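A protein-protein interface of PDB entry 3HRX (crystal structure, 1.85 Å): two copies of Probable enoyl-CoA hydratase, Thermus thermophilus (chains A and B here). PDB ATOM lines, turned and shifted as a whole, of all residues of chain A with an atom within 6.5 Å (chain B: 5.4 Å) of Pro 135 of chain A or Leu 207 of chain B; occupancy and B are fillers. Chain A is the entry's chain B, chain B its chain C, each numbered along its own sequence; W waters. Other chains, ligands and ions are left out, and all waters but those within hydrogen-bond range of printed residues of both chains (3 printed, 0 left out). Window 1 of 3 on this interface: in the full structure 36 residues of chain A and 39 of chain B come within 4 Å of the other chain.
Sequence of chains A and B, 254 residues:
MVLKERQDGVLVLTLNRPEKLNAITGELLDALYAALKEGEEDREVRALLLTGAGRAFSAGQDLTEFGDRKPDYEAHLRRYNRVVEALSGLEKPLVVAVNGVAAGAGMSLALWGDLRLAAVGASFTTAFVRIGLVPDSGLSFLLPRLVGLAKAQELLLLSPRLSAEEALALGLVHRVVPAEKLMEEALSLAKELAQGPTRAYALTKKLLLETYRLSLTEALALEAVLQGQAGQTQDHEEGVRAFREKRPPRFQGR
The backbone carbonyl oxygen (O) of Val 134 of chain A sits at hydrogen-bond distance from the side-chain amide nitrogen (NE2) of Gln 227 of chain B, 2.8 Å away.
The side-chain amide nitrogen (NE2) of Gln 227 of chain B lies within hydrogen-bond range of the side-chain carboxylate (OD2) of Asp 136 of chain A, at 2.8 Å.
The side-chain carboxylate of Glu 223 of chain B lies within hydrogen-bond range of the backbone NH of Ser 137 of chain A (3.1 Å).
The backbone NH of Gly 138 of chain A is in hydrogen-bond range of the side-chain carboxylate of Glu 223 of chain B.
The side-chain hydroxyl (OG1) of Thr 211 of chain B lies within hydrogen-bond range of the backbone carbonyl oxygen (O) of Ser 140 of chain A (3.1 Å).
The side-chain carboxylate (OE1) of Glu 223 of chain B is in hydrogen-bond range of the side-chain hydroxyl (OG) of Ser 140 of chain A, 2.6 Å away.
O of Asp 136 of chain A sits at hydrogen-bond distance from OG of Ser 108 of chain A, at 2.9 Å.
The backbone carbonyl oxygen (O) of Phe 128 of chain A lies within hydrogen-bond range of the backbone NH (N) of Leu 133 of chain A (3.1 Å).
The side-chain carboxylate (OD1) of Asp 136 of chain A lies within hydrogen-bond range of the side-chain hydroxyl (OG) of Ser 137 of chain A.
Among the printed residues, pairs that only touch across the chains: Leu 133 of chain A with Gln 227 of chain B, Val 134 of chain A with Leu 203 of chain B, Val 134 of chain A with Thr 204 of chain B, Val 134 of chain A with Leu 207 of chain B, Pro 135 of chain A with Thr 204 of chain B, Pro 135 of chain A with Leu 207 of chain B, Pro 135 of chain A with Glu 223 of chain B, Asp 136 of chain A with Glu 223 of chain B, Leu 139 of chain A with Glu 223 of chain B, Ser 140 of chain A with Leu 207 of chain B and Leu 156 of chain A with Leu 208 of chain B.
Of the printed residues of chain B, Pro 135 of chain A touches Thr 204 (3.6 Å), Leu 207 (3.8 Å) and Glu 223 (3.7 Å).
Leu 207 of chain B touches three residues of chain A.
Of the printed residues of chain A, Gln 227 of chain B touches Leu 133 (3.3 Å), Val 134 (2.8 Å) and Asp 136 (2.8 Å).
Of the printed residues of chain B, Gly 138 of chain A touches Glu 223 (2.8 Å).
Leu 226 of chain B touches none of the printed residues of chain A.
Leu 222 of chain B touches none of the printed residues of chain A.
The nearest printed residue of chain B that does not touch Ser 140 of chain A is Leu 208 of chain B (4.5 Å).
Hydrophobic or aromatic side chains of chain B within 4 Å of the printed part of chain A: Leu 203, Leu 207 and Leu 208.
Of the 13 printed residues of chain A, 9 touch a printed residue of chain B.
Among the printed residues, no Asp or Glu carboxylate lies within 4 Å of a Lys or Arg side-chain nitrogen of the other chain.
No position is printed for both chains.
Of the 17 pairs that touch across the chains among the printed residues, none has its exchanged pair printed and touching as well.
Water W3 bridges OG of Ser 140 of chain A (2.7 Å) and OG1 of Thr 211 of chain B (3.0 Å).
Water W1 bridges O of Leu 133 of chain A (2.7 Å) and OG1 of Thr 204 of chain B (2.8 Å).
Water W2 lies within hydrogen-bond range of the side-chain carboxylate (OE2) of Glu 223 of chain B (2.8 Å) and the backbone NH (N) of Ser 137 of chain A (2.9 Å).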
ATOM      1  N   SER A 108      -5.049  11.597 -24.613  1.00  0.00           N
ATOM      2  CA  SER A 108      -4.972  10.155 -24.845  1.00  0.00           C
ATOM      3  C   SER A 108      -5.299   9.848 -26.305  1.00  0.00           C
ATOM      4  O   SER A 108      -4.555   9.145 -26.990  1.00  0.00           O
ATOM      5  CB  SER A 108      -5.962   9.409 -23.944  1.00  0.00           C
ATOM      6  OG  SER A 108      -5.749   9.700 -22.574  1.00  0.00           O
ATOM      7  N   THR A 126      -1.723  16.331 -19.354  1.00  0.00           N
ATOM      8  CA  THR A 126      -2.275  15.043 -18.939  1.00  0.00           C
ATOM      9  C   THR A 126      -3.597  15.274 -18.204  1.00  0.00           C
ATOM     10  O   THR A 126      -4.561  14.528 -18.382  1.00  0.00           O
ATOM     11  CB  THR A 126      -1.289  14.267 -18.054  1.00  0.00           C
ATOM     12  OG1 THR A 126      -0.921  15.064 -16.924  1.00  0.00           O
ATOM     13  CG2 THR A 126      -0.037  13.907 -18.860  1.00  0.00           C
ATOM     14  N   PHE A 128      -5.560  14.514 -15.893  1.00  0.00           N
ATOM     15  CA  PHE A 128      -6.258  13.604 -14.986  1.00  0.00           C
ATOM     16  C   PHE A 128      -5.985  13.826 -13.500  1.00  0.00           C
ATOM     17  O   PHE A 128      -6.917  13.932 -12.701  1.00  0.00           O
ATOM     18  CB  PHE A 128      -5.940  12.141 -15.320  1.00  0.00           C
ATOM     19  CG  PHE A 128      -6.494  11.681 -16.638  1.00  0.00           C
ATOM     20  CD1 PHE A 128      -5.679  11.611 -17.764  1.00  0.00           C
ATOM     21  CD2 PHE A 128      -7.828  11.299 -16.749  1.00  0.00           C
ATOM     22  CE1 PHE A 128      -6.186  11.162 -18.983  1.00  0.00           C
ATOM     23  CE2 PHE A 128      -8.345  10.850 -17.964  1.00  0.00           C
ATOM     24  CZ  PHE A 128      -7.521  10.781 -19.083  1.00  0.00           C
ATOM     25  N   VAL A 129      -4.712  13.887 -13.128  1.00  0.00           N
ATOM     26  CA  VAL A 129      -4.348  14.055 -11.726  1.00  0.00           C
ATOM     27  C   VAL A 129      -4.947  15.305 -11.081  1.00  0.00           C
ATOM     28  O   VAL A 129      -5.179  15.330  -9.871  1.00  0.00           O
ATOM     29  CB  VAL A 129      -2.813  14.076 -11.550  1.00  0.00           C
ATOM     30  CG1 VAL A 129      -2.241  15.409 -12.015  1.00  0.00           C
ATOM     31  CG2 VAL A 129      -2.453  13.798 -10.105  1.00  0.00           C
ATOM     32  N   LEU A 133      -7.825  11.821 -10.683  1.00  0.00           N
ATOM     33  CA  LEU A 133      -7.968  10.601 -11.472  1.00  0.00           C
ATOM     34  C   LEU A 133      -6.631  10.110 -12.017  1.00  0.00           C
ATOM     35  O   LEU A 133      -5.624  10.816 -11.962  1.00  0.00           O
ATOM     36  CB  LEU A 133      -8.925  10.831 -12.646  1.00  0.00           C
ATOM     37  CG  LEU A 133     -10.374  11.195 -12.310  1.00  0.00           C
ATOM     38  CD1 LEU A 133     -11.167  11.336 -13.596  1.00  0.00           C
ATOM     39  CD2 LEU A 133     -10.982  10.116 -11.420  1.00  0.00           C
ATOM     40  N   VAL A 134      -6.631   8.888 -12.538  1.00  0.00           N
ATOM     41  CA  VAL A 134      -5.430   8.309 -13.122  1.00  0.00           C
ATOM     42  C   VAL A 134      -5.567   8.455 -14.630  1.00  0.00           C
ATOM     43  O   VAL A 134      -6.646   8.757 -15.136  1.00  0.00           O
ATOM     44  CB  VAL A 134      -5.293   6.803 -12.785  1.00  0.00           C
ATOM     45  CG1 VAL A 134      -5.297   6.603 -11.281  1.00  0.00           C
ATOM     46  CG2 VAL A 134      -6.422   6.012 -13.434  1.00  0.00           C
ATOM     47  N   PRO A 135      -4.471   8.265 -15.372  1.00  0.00           N
ATOM     48  CA  PRO A 135      -4.601   8.396 -16.824  1.00  0.00           C
ATOM     49  C   PRO A 135      -5.383   7.214 -17.390  1.00  0.00           C
ATOM     50  O   PRO A 135      -5.192   6.076 -16.955  1.00  0.00           O
ATOM     51  CB  PRO A 135      -3.150   8.413 -17.294  1.00  0.00           C
ATOM     52  CG  PRO A 135      -2.452   7.574 -16.264  1.00  0.00           C
ATOM     53  CD  PRO A 135      -3.070   8.055 -14.978  1.00  0.00           C
ATOM     54  N   ASP A 136      -6.283   7.478 -18.333  1.00  0.00           N
ATOM     55  CA  ASP A 136      -7.031   6.390 -18.944  1.00  0.00           C
ATOM     56  C   ASP A 136      -7.054   6.514 -20.460  1.00  0.00           C
ATOM     57  O   ASP A 136      -6.299   7.305 -21.045  1.00  0.00           O
ATOM     58  CB  ASP A 136      -8.469   6.269 -18.371  1.00  0.00           C
ATOM     59  CG  ASP A 136      -9.368   7.471 -18.681  1.00  0.00           C
ATOM     60  OD1 ASP A 136      -9.331   8.006 -19.809  1.00  0.00           O
ATOM     61  OD2 ASP A 136     -10.151   7.859 -17.782  1.00  0.00           O
ATOM     62  N   SER A 137      -7.898   5.708 -21.090  1.00  0.00           N
ATOM     63  CA  SER A 137      -8.032   5.706 -22.540  1.00  0.00           C
ATOM     64  C   SER A 137      -6.706   5.375 -23.219  1.00  0.00           C
ATOM     65  O   SER A 137      -6.430   5.840 -24.326  1.00  0.00           O
ATOM     66  CB  SER A 137      -8.552   7.062 -23.022  1.00  0.00           C
ATOM     67  OG  SER A 137      -9.813   7.347 -22.433  1.00  0.00           O
ATOM     68  N   GLY A 138      -5.890   4.569 -22.540  1.00  0.00           N
ATOM     69  CA  GLY A 138      -4.609   4.162 -23.089  1.00  0.00           C
ATOM     70  C   GLY A 138      -3.416   5.053 -22.782  1.00  0.00           C
ATOM     71  O   GLY A 138      -2.284   4.719 -23.142  1.00  0.00           O
ATOM     72  N   LEU A 139      -3.641   6.173 -22.106  1.00  0.00           N
ATOM     73  CA  LEU A 139      -2.531   7.075 -21.801  1.00  0.00           C
ATOM     74  C   LEU A 139      -1.426   6.436 -20.950  1.00  0.00           C
ATOM     75  O   LEU A 139      -0.248   6.699 -21.180  1.00  0.00           O
ATOM     76  CB  LEU A 139      -3.041   8.351 -21.120  1.00  0.00           C
ATOM     77  CG  LEU A 139      -1.988   9.458 -20.951  1.00  0.00           C
ATOM     78  CD1 LEU A 139      -1.442   9.872 -22.317  1.00  0.00           C
ATOM     79  CD2 LEU A 139      -2.604  10.654 -20.239  1.00  0.00           C
ATOM     80  N   SER A 140      -1.791   5.597 -19.980  1.00  0.00           N
ATOM     81  CA  SER A 140      -0.772   4.963 -19.133  1.00  0.00           C
ATOM     82  C   SER A 140       0.059   3.971 -19.943  1.00  0.00           C
ATOM     83  O   SER A 140       1.185   3.643 -19.573  1.00  0.00           O
ATOM     84  CB  SER A 140      -1.419   4.241 -17.940  1.00  0.00           C
ATOM     85  OG  SER A 140      -2.033   3.024 -18.335  1.00  0.00           O
ATOM     86  N   LEU A 156       2.606  12.980 -15.848  1.00  0.00           N
ATOM     87  CA  LEU A 156       1.406  12.446 -15.216  1.00  0.00           C
ATOM     88  C   LEU A 156       1.192  12.910 -13.778  1.00  0.00           C
ATOM     89  O   LEU A 156       0.075  13.251 -13.390  1.00  0.00           O
ATOM     90  CB  LEU A 156       1.437  10.917 -15.251  1.00  0.00           C
ATOM     91  CG  LEU A 156       1.278  10.269 -16.629  1.00  0.00           C
ATOM     92  CD1 LEU A 156       1.544   8.774 -16.534  1.00  0.00           C
ATOM     93  CD2 LEU A 156      -0.130  10.530 -17.152  1.00  0.00           C
ATOM     94  N   LEU B 203      -2.250   5.151  -7.480  1.00  0.00           N
ATOM     95  CA  LEU B 203      -2.759   4.310  -8.551  1.00  0.00           C
ATOM     96  C   LEU B 203      -2.059   4.569  -9.878  1.00  0.00           C
ATOM     97  O   LEU B 203      -1.930   3.658 -10.702  1.00  0.00           O
ATOM     98  CB  LEU B 203      -4.267   4.511  -8.696  1.00  0.00           C
ATOM     99  CG  LEU B 203      -5.074   4.176  -7.434  1.00  0.00           C
ATOM    100  CD1 LEU B 203      -6.543   4.474  -7.668  1.00  0.00           C
ATOM    101  CD2 LEU B 203      -4.877   2.713  -7.071  1.00  0.00           C
ATOM    102  N   THR B 204      -1.608   5.802 -10.086  1.00  0.00           N
ATOM    103  CA  THR B 204      -0.906   6.140 -11.322  1.00  0.00           C
ATOM    104  C   THR B 204       0.430   5.393 -11.320  1.00  0.00           C
ATOM    105  O   THR B 204       0.841   4.830 -12.337  1.00  0.00           O
ATOM    106  CB  THR B 204      -0.659   7.670 -11.436  1.00  0.00           C
ATOM    107  OG1 THR B 204      -1.914   8.350 -11.583  1.00  0.00           O
ATOM    108  CG2 THR B 204       0.225   7.991 -12.638  1.00  0.00           C
ATOM    109  N   LYS B 205       1.096   5.380 -10.167  1.00  0.00           N
ATOM    110  CA  LYS B 205       2.380   4.695 -10.023  1.00  0.00           C
ATOM    111  C   LYS B 205       2.217   3.211 -10.322  1.00  0.00           C
ATOM    112  O   LYS B 205       3.077   2.593 -10.952  1.00  0.00           O
ATOM    113  CB  LYS B 205       2.928   4.873  -8.602  1.00  0.00           C
ATOM    114  CG  LYS B 205       3.396   6.288  -8.302  1.00  0.00           C
ATOM    115  CD  LYS B 205       3.808   6.471  -6.845  1.00  0.00           C
ATOM    116  CE  LYS B 205       4.944   5.543  -6.447  1.00  0.00           C
ATOM    117  NZ  LYS B 205       5.620   6.025  -5.207  1.00  0.00           N
ATOM    118  N   LYS B 206       1.102   2.646  -9.869  1.00  0.00           N
ATOM    119  CA  LYS B 206       0.818   1.237 -10.087  1.00  0.00           C
ATOM    120  C   LYS B 206       0.708   0.948 -11.584  1.00  0.00           C
ATOM    121  O   LYS B 206       1.253  -0.043 -12.068  1.00  0.00           O
ATOM    122  CB  LYS B 206      -0.483   0.863  -9.372  1.00  0.00           C
ATOM    123  CG  LYS B 206      -0.911  -0.586  -9.511  1.00  0.00           C
ATOM    124  CD  LYS B 206      -2.131  -0.858  -8.630  1.00  0.00           C
ATOM    125  CE  LYS B 206      -2.708  -2.249  -8.870  1.00  0.00           C
ATOM    126  NZ  LYS B 206      -1.693  -3.318  -8.656  1.00  0.00           N
ATOM    127  N   LEU B 207       0.009   1.815 -12.312  1.00  0.00           N
ATOM    128  CA  LEU B 207      -0.148   1.633 -13.755  1.00  0.00           C
ATOM    129  C   LEU B 207       1.200   1.689 -14.469  1.00  0.00           C
ATOM    130  O   LEU B 207       1.477   0.877 -15.357  1.00  0.00           O
ATOM    131  CB  LEU B 207      -1.075   2.711 -14.341  1.00  0.00           C
ATOM    132  CG  LEU B 207      -2.578   2.620 -14.044  1.00  0.00           C
ATOM    133  CD1 LEU B 207      -3.279   3.896 -14.490  1.00  0.00           C
ATOM    134  CD2 LEU B 207      -3.166   1.413 -14.756  1.00  0.00           C
ATOM    135  N   LEU B 208       2.037   2.647 -14.078  1.00  0.00           N
ATOM    136  CA  LEU B 208       3.345   2.811 -14.702  1.00  0.00           C
ATOM    137  C   LEU B 208       4.269   1.633 -14.447  1.00  0.00           C
ATOM    138  O   LEU B 208       4.987   1.190 -15.341  1.00  0.00           O
ATOM    139  CB  LEU B 208       4.012   4.105 -14.220  1.00  0.00           C
ATOM    140  CG  LEU B 208       3.361   5.403 -14.713  1.00  0.00           C
ATOM    141  CD1 LEU B 208       3.971   6.603 -14.009  1.00  0.00           C
ATOM    142  CD2 LEU B 208       3.533   5.509 -16.223  1.00  0.00           C
ATOM    143  N   LEU B 209       4.244   1.115 -13.227  1.00  0.00           N
ATOM    144  CA  LEU B 209       5.105  -0.002 -12.875  1.00  0.00           C
ATOM    145  C   LEU B 209       4.781  -1.256 -13.684  1.00  0.00           C
ATOM    146  O   LEU B 209       5.668  -2.039 -14.022  1.00  0.00           O
ATOM    147  CB  LEU B 209       4.965  -0.309 -11.379  1.00  0.00           C
ATOM    148  CG  LEU B 209       6.050  -1.174 -10.738  1.00  0.00           C
ATOM    149  CD1 LEU B 209       7.390  -0.465 -10.852  1.00  0.00           C
ATOM    150  CD2 LEU B 209       5.705  -1.431  -9.274  1.00  0.00           C
ATOM    151  N   GLU B 210       3.510  -1.424 -14.018  1.00  0.00           N
ATOM    152  CA  GLU B 210       3.053  -2.614 -14.728  1.00  0.00           C
ATOM    153  C   GLU B 210       2.813  -2.477 -16.226  1.00  0.00           C
ATOM    154  O   GLU B 210       2.507  -3.463 -16.899  1.00  0.00           O
ATOM    155  CB  GLU B 210       1.761  -3.104 -14.059  1.00  0.00           C
ATOM    156  CG  GLU B 210       1.956  -3.573 -12.618  1.00  0.00           C
ATOM    157  CD  GLU B 210       0.664  -3.604 -11.815  1.00  0.00           C
ATOM    158  OE1 GLU B 210      -0.346  -4.139 -12.321  1.00  0.00           O
ATOM    159  OE2 GLU B 210       0.663  -3.099 -10.670  1.00  0.00           O
ATOM    160  N   THR B 211       2.983  -1.275 -16.760  1.00  0.00           N
ATOM    161  CA  THR B 211       2.690  -1.028 -18.163  1.00  0.00           C
ATOM    162  C   THR B 211       3.432  -1.793 -19.264  1.00  0.00           C
ATOM    163  O   THR B 211       2.793  -2.332 -20.166  1.00  0.00           O
ATOM    164  CB  THR B 211       2.778   0.483 -18.474  1.00  0.00           C
ATOM    165  OG1 THR B 211       2.214   0.736 -19.766  1.00  0.00           O
ATOM    166  CG2 THR B 211       4.218   0.959 -18.451  1.00  0.00           C
ATOM    167  N   ALA B 219      -3.868  -3.507 -20.328  1.00  0.00           N
ATOM    168  CA  ALA B 219      -3.623  -2.170 -19.799  1.00  0.00           C
ATOM    169  C   ALA B 219      -4.931  -1.383 -19.706  1.00  0.00           C
ATOM    170  O   ALA B 219      -5.198  -0.732 -18.698  1.00  0.00           O
ATOM    171  CB  ALA B 219      -2.625  -1.428 -20.686  1.00  0.00           C
ATOM    172  N   LEU B 222      -6.931  -2.596 -16.809  1.00  0.00           N
ATOM    173  CA  LEU B 222      -6.391  -2.152 -15.530  1.00  0.00           C
ATOM    174  C   LEU B 222      -6.717  -0.675 -15.312  1.00  0.00           C
ATOM    175  O   LEU B 222      -7.038  -0.266 -14.195  1.00  0.00           O
ATOM    176  CB  LEU B 222      -4.874  -2.379 -15.475  1.00  0.00           C
ATOM    177  CG  LEU B 222      -4.204  -2.081 -14.129  1.00  0.00           C
ATOM    178  CD1 LEU B 222      -4.842  -2.941 -13.033  1.00  0.00           C
ATOM    179  CD2 LEU B 222      -2.711  -2.363 -14.224  1.00  0.00           C
ATOM    180  N   GLU B 223      -6.638   0.125 -16.375  1.00  0.00           N
ATOM    181  CA  GLU B 223      -6.969   1.542 -16.263  1.00  0.00           C
ATOM    182  C   GLU B 223      -8.422   1.661 -15.795  1.00  0.00           C
ATOM    183  O   GLU B 223      -8.745   2.475 -14.931  1.00  0.00           O
ATOM    184  CB  GLU B 223      -6.804   2.254 -17.615  1.00  0.00           C
ATOM    185  CG  GLU B 223      -5.351   2.503 -18.027  1.00  0.00           C
ATOM    186  CD  GLU B 223      -5.226   3.169 -19.395  1.00  0.00           C
ATOM    187  OE1 GLU B 223      -4.112   3.622 -19.745  1.00  0.00           O
ATOM    188  OE2 GLU B 223      -6.237   3.234 -20.124  1.00  0.00           O
ATOM    189  N   LEU B 226      -8.624   0.654 -11.954  1.00  0.00           N
ATOM    190  CA  LEU B 226      -8.053   1.674 -11.080  1.00  0.00           C
ATOM    191  C   LEU B 226      -8.774   3.016 -11.161  1.00  0.00           C
ATOM    192  O   LEU B 226      -8.858   3.738 -10.167  1.00  0.00           O
ATOM    193  CB  LEU B 226      -6.557   1.844 -11.371  1.00  0.00           C
ATOM    194  CG  LEU B 226      -5.748   0.552 -11.186  1.00  0.00           C
ATOM    195  CD1 LEU B 226      -4.259   0.826 -11.387  1.00  0.00           C
ATOM    196  CD2 LEU B 226      -5.996  -0.009  -9.788  1.00  0.00           C
ATOM    197  N   GLN B 227      -9.298   3.357 -12.335  1.00  0.00           N
ATOM    198  CA  GLN B 227     -10.022   4.616 -12.474  1.00  0.00           C
ATOM    199  C   GLN B 227     -11.314   4.491 -11.676  1.00  0.00           C
ATOM    200  O   GLN B 227     -11.781   5.458 -11.075  1.00  0.00           O
ATOM    201  CB  GLN B 227     -10.358   4.901 -13.939  1.00  0.00           C
ATOM    202  CG  GLN B 227     -10.856   6.319 -14.188  1.00  0.00           C
ATOM    203  CD  GLN B 227      -9.763   7.357 -14.000  1.00  0.00           C
ATOM    204  OE1 GLN B 227      -9.295   7.595 -12.886  1.00  0.00           O
ATOM    205  NE2 GLN B 227      -9.337   7.968 -15.100  1.00  0.00           N
HETATM  206  O   HOH W   1      -2.984  10.674 -12.712  1.00  0.00           O
HETATM  207  O   HOH W   2      -8.993   3.223 -20.212  1.00  0.00           O
HETATM  208  O   HOH W   3      -0.606   0.764 -18.618  1.00  0.00           O
